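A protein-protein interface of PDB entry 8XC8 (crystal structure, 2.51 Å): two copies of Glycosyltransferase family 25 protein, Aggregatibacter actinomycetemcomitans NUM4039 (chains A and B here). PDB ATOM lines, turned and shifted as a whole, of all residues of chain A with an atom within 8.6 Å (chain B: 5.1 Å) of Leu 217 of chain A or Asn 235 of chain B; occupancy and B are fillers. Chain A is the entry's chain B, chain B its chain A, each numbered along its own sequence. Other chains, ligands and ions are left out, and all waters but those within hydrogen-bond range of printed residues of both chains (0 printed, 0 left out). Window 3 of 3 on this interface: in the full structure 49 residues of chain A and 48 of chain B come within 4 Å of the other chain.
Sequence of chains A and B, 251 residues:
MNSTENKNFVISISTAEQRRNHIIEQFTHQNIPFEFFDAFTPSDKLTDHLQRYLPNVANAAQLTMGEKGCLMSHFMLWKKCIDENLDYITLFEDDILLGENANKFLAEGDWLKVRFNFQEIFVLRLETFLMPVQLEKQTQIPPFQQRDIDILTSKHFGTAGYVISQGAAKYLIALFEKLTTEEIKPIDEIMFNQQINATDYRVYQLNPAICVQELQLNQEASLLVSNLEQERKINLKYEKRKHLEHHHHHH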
ATOM      1  N   ILE A  96      21.107  -7.445  14.145  1.00  0.00           N
ATOM      2  CA  ILE A  96      19.666  -7.767  13.931  1.00  0.00           C
ATOM      3  C   ILE A  96      19.515  -8.859  12.874  1.00  0.00           C
ATOM      4  O   ILE A  96      20.481  -9.127  12.152  1.00  0.00           O
ATOM      5  CB  ILE A  96      18.842  -6.530  13.547  1.00  0.00           C
ATOM      6  CG1 ILE A  96      19.436  -5.824  12.334  1.00  0.00           C
ATOM      7  CG2 ILE A  96      18.679  -5.579  14.721  1.00  0.00           C
ATOM      8  CD1 ILE A  96      18.398  -5.174  11.456  1.00  0.00           C
ATOM      9  N   LEU A  97      18.329  -9.472  12.849  1.00  0.00           N
ATOM     10  CA  LEU A  97      17.866 -10.467  11.844  1.00  0.00           C
ATOM     11  C   LEU A  97      16.494 -10.015  11.341  1.00  0.00           C
ATOM     12  O   LEU A  97      15.721  -9.529  12.173  1.00  0.00           O
ATOM     13  CB  LEU A  97      17.777 -11.860  12.480  1.00  0.00           C
ATOM     14  CG  LEU A  97      19.034 -12.335  13.209  1.00  0.00           C
ATOM     15  CD1 LEU A  97      18.769 -13.628  13.965  1.00  0.00           C
ATOM     16  CD2 LEU A  97      20.197 -12.503  12.244  1.00  0.00           C
ATOM     17  N   LEU A  98      16.207 -10.171  10.046  1.00  0.00           N
ATOM     18  CA  LEU A  98      14.971  -9.656   9.405  1.00  0.00           C
ATOM     19  C   LEU A  98      13.966 -10.794   9.171  1.00  0.00           C
ATOM     20  O   LEU A  98      14.389 -11.966   9.115  1.00  0.00           O
ATOM     21  CB  LEU A  98      15.353  -8.987   8.085  1.00  0.00           C
ATOM     22  CG  LEU A  98      16.225  -7.734   8.175  1.00  0.00           C
ATOM     23  CD1 LEU A  98      16.258  -7.019   6.830  1.00  0.00           C
ATOM     24  CD2 LEU A  98      15.740  -6.776   9.248  1.00  0.00           C
ATOM     25  N   GLY A  99      12.686 -10.442   8.996  1.00  0.00           N
ATOM     26  CA  GLY A  99      11.567 -11.363   8.706  1.00  0.00           C
ATOM     27  C   GLY A  99      10.974 -11.120   7.326  1.00  0.00           C
ATOM     28  O   GLY A  99      11.335 -10.118   6.689  1.00  0.00           O
ATOM     29  N   THR A 128      11.340  -7.005  18.158  1.00  0.00           N
ATOM     30  CA  THR A 128      10.718  -7.793  19.252  1.00  0.00           C
ATOM     31  C   THR A 128      11.111  -7.189  20.603  1.00  0.00           C
ATOM     32  O   THR A 128      11.826  -6.202  20.606  1.00  0.00           O
ATOM     33  CB  THR A 128      11.198  -9.244  19.188  1.00  0.00           C
ATOM     34  OG1 THR A 128      12.601  -9.198  19.454  1.00  0.00           O
ATOM     35  CG2 THR A 128      10.921  -9.880  17.842  1.00  0.00           C
ATOM     36  N   PHE A 129      10.681  -7.781  21.716  1.00  0.00           N
ATOM     37  CA  PHE A 129      11.080  -7.358  23.083  1.00  0.00           C
ATOM     38  C   PHE A 129      12.337  -8.107  23.532  1.00  0.00           C
ATOM     39  O   PHE A 129      12.518  -9.306  23.220  1.00  0.00           O
ATOM     40  CB  PHE A 129       9.933  -7.552  24.070  1.00  0.00           C
ATOM     41  CG  PHE A 129       8.775  -6.648  23.761  1.00  0.00           C
ATOM     42  CD1 PHE A 129       8.870  -5.286  23.985  1.00  0.00           C
ATOM     43  CD2 PHE A 129       7.622  -7.145  23.185  1.00  0.00           C
ATOM     44  CE1 PHE A 129       7.809  -4.443  23.692  1.00  0.00           C
ATOM     45  CE2 PHE A 129       6.562  -6.301  22.892  1.00  0.00           C
ATOM     46  CZ  PHE A 129       6.655  -4.954  23.149  1.00  0.00           C
ATOM     47  N   MET A 131      14.565  -9.729  26.549  1.00  0.00           N
ATOM     48  CA  MET A 131      14.520 -10.421  27.871  1.00  0.00           C
ATOM     49  C   MET A 131      15.957 -10.622  28.342  1.00  0.00           C
ATOM     50  O   MET A 131      16.805 -11.011  27.543  1.00  0.00           O
ATOM     51  CB  MET A 131      13.859 -11.803  27.787  1.00  0.00           C
ATOM     52  CG  MET A 131      12.395 -11.815  27.411  1.00  0.00           C
ATOM     53  SD  MET A 131      11.240 -10.663  28.505  1.00  0.00           S
ATOM     54  CE  MET A 131      10.322  -9.647  27.098  1.00  0.00           C
ATOM     55  N   CYS A 211      12.129  -7.558  13.094  1.00  0.00           N
ATOM     56  CA  CYS A 211      13.553  -7.836  13.398  1.00  0.00           C
ATOM     57  C   CYS A 211      13.717  -8.286  14.853  1.00  0.00           C
ATOM     58  O   CYS A 211      12.707  -8.282  15.590  1.00  0.00           O
ATOM     59  CB  CYS A 211      14.424  -6.633  13.062  1.00  0.00           C
ATOM     60  SG  CYS A 211      14.049  -5.153  14.033  1.00  0.00           S
ATOM     61  N   VAL A 212      14.937  -8.699  15.213  1.00  0.00           N
ATOM     62  CA  VAL A 212      15.315  -9.272  16.541  1.00  0.00           C
ATOM     63  C   VAL A 212      16.841  -9.263  16.654  1.00  0.00           C
ATOM     64  O   VAL A 212      17.494  -9.524  15.630  1.00  0.00           O
ATOM     65  CB  VAL A 212      14.783 -10.707  16.722  1.00  0.00           C
ATOM     66  CG1 VAL A 212      15.014 -11.567  15.489  1.00  0.00           C
ATOM     67  CG2 VAL A 212      15.391 -11.380  17.947  1.00  0.00           C
ATOM     68  N   GLN A 213      17.372  -9.025  17.856  1.00  0.00           N
ATOM     69  CA  GLN A 213      18.829  -9.102  18.131  1.00  0.00           C
ATOM     70  C   GLN A 213      19.295 -10.553  17.971  1.00  0.00           C
ATOM     71  O   GLN A 213      18.590 -11.480  18.436  1.00  0.00           O
ATOM     72  CB  GLN A 213      19.154  -8.523  19.507  1.00  0.00           C
ATOM     73  CG  GLN A 213      18.652  -7.095  19.692  1.00  0.00           C
ATOM     74  CD  GLN A 213      19.554  -6.231  20.546  1.00  0.00           C
ATOM     75  OE1 GLN A 213      20.776  -6.361  20.516  1.00  0.00           O
ATOM     76  NE2 GLN A 213      18.961  -5.319  21.305  1.00  0.00           N
ATOM     77  N   GLU A 214      20.451 -10.729  17.332  1.00  0.00           N
ATOM     78  CA  GLU A 214      20.953 -12.022  16.790  1.00  0.00           C
ATOM     79  C   GLU A 214      20.678 -13.142  17.800  1.00  0.00           C
ATOM     80  O   GLU A 214      19.976 -14.104  17.448  1.00  0.00           O
ATOM     81  CB  GLU A 214      22.452 -11.929  16.476  1.00  0.00           C
ATOM     82  CG  GLU A 214      22.905 -12.768  15.288  1.00  0.00           C
ATOM     83  CD  GLU A 214      23.838 -12.039  14.322  1.00  0.00           C
ATOM     84  OE1 GLU A 214      24.087 -12.569  13.213  1.00  0.00           O
ATOM     85  OE2 GLU A 214      24.306 -10.932  14.672  1.00  0.00           O
ATOM     86  N   LEU A 215      21.181 -12.992  19.026  1.00  0.00           N
ATOM     87  CA  LEU A 215      21.339 -14.117  19.978  1.00  0.00           C
ATOM     88  C   LEU A 215      20.192 -14.131  20.990  1.00  0.00           C
ATOM     89  O   LEU A 215      20.306 -14.879  21.974  1.00  0.00           O
ATOM     90  CB  LEU A 215      22.694 -13.970  20.677  1.00  0.00           C
ATOM     91  CG  LEU A 215      23.541 -15.242  20.683  1.00  0.00           C
ATOM     92  CD1 LEU A 215      24.190 -15.458  19.321  1.00  0.00           C
ATOM     93  CD2 LEU A 215      24.584 -15.196  21.787  1.00  0.00           C
ATOM     94  N   GLN A 216      19.134 -13.350  20.759  1.00  0.00           N
ATOM     95  CA  GLN A 216      18.046 -13.135  21.744  1.00  0.00           C
ATOM     96  C   GLN A 216      17.375 -14.481  22.020  1.00  0.00           C
ATOM     97  O   GLN A 216      17.179 -14.809  23.209  1.00  0.00           O
ATOM     98  CB  GLN A 216      17.051 -12.096  21.228  1.00  0.00           C
ATOM     99  CG  GLN A 216      16.018 -11.649  22.255  1.00  0.00           C
ATOM    100  CD  GLN A 216      16.574 -11.032  23.519  1.00  0.00           C
ATOM    101  OE1 GLN A 216      15.911 -11.024  24.555  1.00  0.00           O
ATOM    102  NE2 GLN A 216      17.777 -10.482  23.446  1.00  0.00           N
ATOM    103  N   LEU A 217      17.078 -15.235  20.959  1.00  0.00           N
ATOM    104  CA  LEU A 217      16.428 -16.567  21.042  1.00  0.00           C
ATOM    105  C   LEU A 217      17.223 -17.479  21.983  1.00  0.00           C
ATOM    106  O   LEU A 217      16.650 -17.937  22.984  1.00  0.00           O
ATOM    107  CB  LEU A 217      16.339 -17.173  19.640  1.00  0.00           C
ATOM    108  CG  LEU A 217      15.777 -18.592  19.570  1.00  0.00           C
ATOM    109  CD1 LEU A 217      14.445 -18.684  20.293  1.00  0.00           C
ATOM    110  CD2 LEU A 217      15.628 -19.053  18.130  1.00  0.00           C
ATOM    111  N   ASN A 218      18.500 -17.721  21.670  1.00  0.00           N
ATOM    112  CA  ASN A 218      19.385 -18.636  22.441  1.00  0.00           C
ATOM    113  C   ASN A 218      19.296 -18.259  23.921  1.00  0.00           C
ATOM    114  O   ASN A 218      19.194 -19.166  24.770  1.00  0.00           O
ATOM    115  CB  ASN A 218      20.846 -18.586  21.983  1.00  0.00           C
ATOM    116  CG  ASN A 218      21.012 -18.300  20.503  1.00  0.00           C
ATOM    117  OD1 ASN A 218      20.353 -17.412  19.956  1.00  0.00           O
ATOM    118  ND2 ASN A 218      21.907 -19.024  19.850  1.00  0.00           N
ATOM    119  N   GLN A 219      19.327 -16.952  24.194  1.00  0.00           N
ATOM    120  CA  GLN A 219      19.300 -16.378  25.556  1.00  0.00           C
ATOM    121  C   GLN A 219      17.907 -16.550  26.158  1.00  0.00           C
ATOM    122  O   GLN A 219      17.833 -17.009  27.305  1.00  0.00           O
ATOM    123  CB  GLN A 219      19.676 -14.902  25.530  1.00  0.00           C
ATOM    124  CG  GLN A 219      20.217 -14.432  26.869  1.00  0.00           C
ATOM    125  CD  GLN A 219      19.619 -13.117  27.300  1.00  0.00           C
ATOM    126  OE1 GLN A 219      19.413 -12.206  26.495  1.00  0.00           O
ATOM    127  NE2 GLN A 219      19.331 -13.020  28.587  1.00  0.00           N
ATOM    128  N   GLU A 220      16.854 -16.174  25.429  1.00  0.00           N
ATOM    129  CA  GLU A 220      15.438 -16.385  25.849  1.00  0.00           C
ATOM    130  C   GLU A 220      15.256 -17.841  26.306  1.00  0.00           C
ATOM    131  O   GLU A 220      14.805 -18.053  27.438  1.00  0.00           O
ATOM    132  CB  GLU A 220      14.485 -16.040  24.702  1.00  0.00           C
ATOM    133  CG  GLU A 220      13.082 -15.666  25.146  1.00  0.00           C
ATOM    134  CD  GLU A 220      12.603 -14.250  24.850  1.00  0.00           C
ATOM    135  OE1 GLU A 220      11.399 -13.970  25.119  1.00  0.00           O
ATOM    136  OE2 GLU A 220      13.415 -13.423  24.360  1.00  0.00           O
ATOM    137  N   ALA A 221      15.614 -18.809  25.465  1.00  0.00           N
ATOM    138  CA  ALA A 221      15.549 -20.261  25.763  1.00  0.00           C
ATOM    139  C   ALA A 221      16.381 -20.571  27.012  1.00  0.00           C
ATOM    140  O   ALA A 221      15.874 -21.235  27.920  1.00  0.00           O
ATOM    141  CB  ALA A 221      16.041 -21.059  24.579  1.00  0.00           C
ATOM    142  N   SER A 222      17.630 -20.107  27.044  1.00  0.00           N
ATOM    143  CA  SER A 222      18.576 -20.353  28.160  1.00  0.00           C
ATOM    144  C   SER A 222      17.971 -19.857  29.481  1.00  0.00           C
ATOM    145  O   SER A 222      18.215 -20.515  30.508  1.00  0.00           O
ATOM    146  CB  SER A 222      19.911 -19.725  27.895  1.00  0.00           C
ATOM    147  OG  SER A 222      20.631 -19.571  29.108  1.00  0.00           O
ATOM    148  N   LEU A 223      17.213 -18.756  29.450  1.00  0.00           N
ATOM    149  CA  LEU A 223      16.573 -18.146  30.646  1.00  0.00           C
ATOM    150  C   LEU A 223      15.570 -19.117  31.259  1.00  0.00           C
ATOM    151  O   LEU A 223      15.564 -19.225  32.516  1.00  0.00           O
ATOM    152  CB  LEU A 223      15.856 -16.849  30.269  1.00  0.00           C
ATOM    153  CG  LEU A 223      16.727 -15.597  30.172  1.00  0.00           C
ATOM    154  CD1 LEU A 223      15.914 -14.425  29.642  1.00  0.00           C
ATOM    155  CD2 LEU A 223      17.339 -15.245  31.518  1.00  0.00           C
ATOM    156  N   LEU A 224      14.749 -19.754  30.420  1.00  0.00           N
ATOM    157  CA  LEU A 224      13.659 -20.665  30.862  1.00  0.00           C
ATOM    158  C   LEU A 224      14.220 -22.015  31.291  1.00  0.00           C
ATOM    159  O   LEU A 224      13.649 -22.619  32.212  1.00  0.00           O
ATOM    160  CB  LEU A 224      12.684 -20.887  29.708  1.00  0.00           C
ATOM    161  CG  LEU A 224      11.676 -19.767  29.505  1.00  0.00           C
ATOM    162  CD1 LEU A 224      10.831 -20.011  28.267  1.00  0.00           C
ATOM    163  CD2 LEU A 224      10.804 -19.611  30.740  1.00  0.00           C
ATOM    164  N   VAL A 225      15.235 -22.490  30.581  1.00  0.00           N
ATOM    165  CA  VAL A 225      15.743 -23.878  30.745  1.00  0.00           C
ATOM    166  C   VAL A 225      16.585 -23.936  32.015  1.00  0.00           C
ATOM    167  O   VAL A 225      16.457 -24.919  32.747  1.00  0.00           O
ATOM    168  CB  VAL A 225      16.529 -24.356  29.517  1.00  0.00           C
ATOM    169  CG1 VAL A 225      17.226 -25.677  29.792  1.00  0.00           C
ATOM    170  CG2 VAL A 225      15.632 -24.464  28.293  1.00  0.00           C
ATOM    171  N   LEU B 228       8.103 -14.453  21.712  1.00  0.00           N
ATOM    172  CA  LEU B 228       9.068 -15.583  21.615  1.00  0.00           C
ATOM    173  C   LEU B 228       8.877 -16.330  20.286  1.00  0.00           C
ATOM    174  O   LEU B 228       9.879 -16.516  19.588  1.00  0.00           O
ATOM    175  CB  LEU B 228       8.905 -16.486  22.842  1.00  0.00           C
ATOM    176  CG  LEU B 228       9.673 -17.806  22.806  1.00  0.00           C
ATOM    177  CD1 LEU B 228      11.118 -17.596  22.413  1.00  0.00           C
ATOM    178  CD2 LEU B 228       9.598 -18.507  24.149  1.00  0.00           C
ATOM    179  N   GLU B 231      10.142 -14.390  17.365  1.00  0.00           N
ATOM    180  CA  GLU B 231      11.631 -14.451  17.442  1.00  0.00           C
ATOM    181  C   GLU B 231      12.135 -15.764  16.838  1.00  0.00           C
ATOM    182  O   GLU B 231      13.118 -15.710  16.086  1.00  0.00           O
ATOM    183  CB  GLU B 231      12.142 -14.380  18.885  1.00  0.00           C
ATOM    184  CG  GLU B 231      12.303 -12.974  19.441  1.00  0.00           C
ATOM    185  CD  GLU B 231      12.975 -12.907  20.808  1.00  0.00           C
ATOM    186  OE1 GLU B 231      13.744 -13.837  21.132  1.00  0.00           O
ATOM    187  OE2 GLU B 231      12.728 -11.929  21.552  1.00  0.00           O
ATOM    188  N   ARG B 232      11.502 -16.891  17.183  1.00  0.00           N
ATOM    189  CA  ARG B 232      11.910 -18.244  16.719  1.00  0.00           C
ATOM    190  C   ARG B 232      11.791 -18.331  15.195  1.00  0.00           C
ATOM    191  O   ARG B 232      12.737 -18.851  14.550  1.00  0.00           O
ATOM    192  CB  ARG B 232      11.044 -19.343  17.338  1.00  0.00           C
ATOM    193  CG  ARG B 232      11.417 -20.745  16.877  1.00  0.00           C
ATOM    194  CD  ARG B 232      10.511 -21.816  17.454  1.00  0.00           C
ATOM    195  NE  ARG B 232       9.275 -21.947  16.698  1.00  0.00           N
ATOM    196  CZ  ARG B 232       9.169 -22.522  15.504  1.00  0.00           C
ATOM    197  NH1 ARG B 232      10.232 -23.040  14.903  1.00  0.00           N
ATOM    198  NH2 ARG B 232       7.989 -22.571  14.908  1.00  0.00           N
ATOM    199  N   LYS B 233      10.659 -17.880  14.653  1.00  0.00           N
ATOM    200  CA  LYS B 233      10.338 -18.016  13.210  1.00  0.00           C
ATOM    201  C   LYS B 233      11.343 -17.173  12.417  1.00  0.00           C
ATOM    202  O   LYS B 233      11.815 -17.667  11.383  1.00  0.00           O
ATOM    203  CB  LYS B 233       8.864 -17.690  12.933  1.00  0.00           C
ATOM    204  CG  LYS B 233       7.933 -18.905  12.944  1.00  0.00           C
ATOM    205  CD  LYS B 233       6.433 -18.596  12.935  1.00  0.00           C
ATOM    206  CE  LYS B 233       5.570 -19.758  13.414  1.00  0.00           C
ATOM    207  NZ  LYS B 233       4.166 -19.372  13.724  1.00  0.00           N
ATOM    208  N   ILE B 234      11.712 -15.988  12.911  1.00  0.00           N
ATOM    209  CA  ILE B 234      12.710 -15.092  12.247  1.00  0.00           C
ATOM    210  C   ILE B 234      14.097 -15.751  12.249  1.00  0.00           C
ATOM    211  O   ILE B 234      14.813 -15.597  11.248  1.00  0.00           O
ATOM    212  CB  ILE B 234      12.754 -13.702  12.907  1.00  0.00           C
ATOM    213  CG1 ILE B 234      11.443 -12.939  12.714  1.00  0.00           C
ATOM    214  CG2 ILE B 234      13.947 -12.914  12.387  1.00  0.00           C
ATOM    215  CD1 ILE B 234      11.429 -11.565  13.343  1.00  0.00           C
ATOM    216  N   ASN B 235      14.486 -16.408  13.346  1.00  0.00           N
ATOM    217  CA  ASN B 235      15.766 -17.159  13.458  1.00  0.00           C
ATOM    218  C   ASN B 235      15.740 -18.296  12.436  1.00  0.00           C
ATOM    219  O   ASN B 235      16.759 -18.503  11.751  1.00  0.00           O
ATOM    220  CB  ASN B 235      16.017 -17.686  14.875  1.00  0.00           C
ATOM    221  CG  ASN B 235      16.751 -16.697  15.762  1.00  0.00           C
ATOM    222  OD1 ASN B 235      16.154 -15.770  16.315  1.00  0.00           O
ATOM    223  ND2 ASN B 235      18.051 -16.893  15.920  1.00  0.00           N
ATOM    224  N   LEU B 236      14.599 -18.981  12.330  1.00  0.00           N
ATOM    225  CA  LEU B 236      14.386 -20.103  11.380  1.00  0.00           C
ATOM    226  C   LEU B 236      14.464 -19.592   9.933  1.00  0.00           C
ATOM    227  O   LEU B 236      15.171 -20.227   9.134  1.00  0.00           O
ATOM    228  CB  LEU B 236      13.035 -20.756  11.678  1.00  0.00           C
ATOM    229  CG  LEU B 236      12.806 -22.099  10.990  1.00  0.00           C
ATOM    230  CD1 LEU B 236      13.698 -23.170  11.598  1.00  0.00           C
ATOM    231  CD2 LEU B 236      11.338 -22.506  11.063  1.00  0.00           C
ATOM    232  N   LYS B 237      13.764 -18.499   9.604  1.00  0.00           N
ATOM    233  CA  LYS B 237      13.865 -17.813   8.283  1.00  0.00           C
ATOM    234  C   LYS B 237      15.343 -17.666   7.922  1.00  0.00           C
ATOM    235  O   LYS B 237      15.784 -18.330   6.973  1.00  0.00           O
ATOM    236  CB  LYS B 237      13.220 -16.421   8.284  1.00  0.00           C
ATOM    237  CG  LYS B 237      11.786 -16.348   7.767  1.00  0.00           C
ATOM    238  CD  LYS B 237      10.739 -16.029   8.829  1.00  0.00           C
ATOM    239  CE  LYS B 237       9.347 -15.856   8.255  1.00  0.00           C
ATOM    240  NZ  LYS B 237       8.386 -15.343   9.260  1.00  0.00           N
ATOM    241  N   TYR B 238      16.078 -16.864   8.695  1.00  0.00           N
ATOM    242  CA  TYR B 238      17.486 -16.466   8.424  1.00  0.00           C
ATOM    243  C   TYR B 238      18.389 -17.696   8.252  1.00  0.00           C
ATOM    244  O   TYR B 238      19.498 -17.505   7.723  1.00  0.00           O
ATOM    245  CB  TYR B 238      18.007 -15.537   9.522  1.00  0.00           C
ATOM    246  CG  TYR B 238      19.481 -15.213   9.443  1.00  0.00           C
ATOM    247  CD1 TYR B 238      20.004 -14.449   8.411  1.00  0.00           C
ATOM    248  CD2 TYR B 238      20.362 -15.663  10.414  1.00  0.00           C
ATOM    249  CE1 TYR B 238      21.359 -14.150   8.340  1.00  0.00           C
ATOM    250  CE2 TYR B 238      21.717 -15.366  10.364  1.00  0.00           C
ATOM    251  CZ  TYR B 238      22.223 -14.608   9.322  1.00  0.00           C
ATOM    252  OH  TYR B 238      23.558 -14.319   9.283  1.00  0.00           O
ATOM    253  N   GLU B 239      17.954 -18.903   8.639  1.00  0.00           N
ATOM    254  CA  GLU B 239      18.739 -20.151   8.423  1.00  0.00           C
ATOM    255  C   GLU B 239      18.494 -20.682   7.006  1.00  0.00           C
ATOM    256  O   GLU B 239      17.958 -21.798   6.885  1.00  0.00           O
ATOM    257  CB  GLU B 239      18.404 -21.207   9.473  1.00  0.00           C
ATOM    258  CG  GLU B 239      18.922 -20.857  10.850  1.00  0.00           C
ATOM    259  CD  GLU B 239      18.253 -21.647  11.957  1.00  0.00           C
ATOM    260  OE1 GLU B 239      18.206 -22.893  11.845  1.00  0.00           O
ATOM    261  OE2 GLU B 239      17.767 -21.016  12.917  1.00  0.00           O
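O of Phe 129 of chain A sits close to OE2 of Glu 231 of chain B, at 3.1 Å.
OE2 of Glu 220 of chain A lies close to OE2 of Glu 231 of chain B (3.3 Å).
OG1 of Thr 128 of chain A is in hydrogen-bond range of OE2 of Glu 231 of chain B (3.4 Å).
No position is printed for both chains.
Of the 14 pairs that touch across the chains among the printed residues, none has its exchanged pair printed and touching as well.
Among the printed residues, pairs that only touch across the chains: Gln 216 of chain A with Glu 231 of chain B (3.3 Å), Leu 98 of chain A with Ile 234 of chain B (3.4 Å), Leu 217 of chain A with Asn 235 of chain B (3.5 Å), Val 212 of chain A with Ile 234 of chain B (3.5 Å), Leu 217 of chain A with Glu 231 of chain B (3.6 Å), Leu 97 of chain A with Tyr 238 of chain B (3.7 Å), Glu 214 of chain A with Asn 235 of chain B (3.7 Å), Val 212 of chain A with Glu 231 of chain B (3.8 Å), Leu 97 of chain A with Ile 234 of chain B (3.8 Å), Leu 97 of chain A with Asn 235 of chain B (3.9 Å) and Glu 220 of chain A with Leu 228 of chain B (3.9 Å).
Printed residues of chain B within 4 Å of Leu 98 of chain A: Ile 234 (3.4 Å).
Printed residues of chain B within 4 Å of Phe 129 of chain A: Glu 231 (3.1 Å).
Printed residues of chain B within 4 Å of Val 212 of chain A: Glu 231 and Ile 234.
Leu 217 of chain A touches two residues of chain B.
Printed residues of chain B within 4 Å of Glu 220 of chain A: Leu 228 (3.9 Å) and Glu 231 (3.3 Å).
Asn 235 of chain B touches just these residues of chain A: Leu 97, Glu 214 and Leu 217.
The nearest residue of chain A that does not touch Asn 235 of chain B is Val 212 of chain A (4.4 Å).
The nearest printed residue of chain B that does not touch Glu 214 of chain A is Tyr 238 of chain B (4.3 Å).
N of Met 131 of chain A lies within hydrogen-bond range of OE1 of Gln 216 of chain A, 2.7 Å away.
OE1 of Gln 216 of chain A lies close to OE2 of Glu 220 of chain A (3.5 Å).
N of Leu 97 of chain A is in hydrogen-bond range of O of Val 212 of chain A, at 2.9 Å.
The backbone carbonyl oxygen of Glu 231 of chain B lies close to the side-chain amide oxygen of Asn 235 of chain B, 3.0 Å away.
The backbone NH (N) of Thr 128 of chain A lies within hydrogen-bond range of the backbone carbonyl oxygen (O) of Cys 211 of chain A, at 3.2 Å.
Hydrophobic or aromatic side chains of chain A that line the printed part of chain B: Leu 97, Val 212 and Leu 217.
Printed residues of chain B that touch a printed residue of chain A: Leu 228, Glu 231, Ile 234, Asn 235 and Tyr 238.
Along chain B the printed residues that touch a printed residue of chain A span positions 228 to 238.
Among the printed residues, no Asp or Glu carboxylate lies within 4 Å of a Lys or Arg side-chain nitrogen of the other chain.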
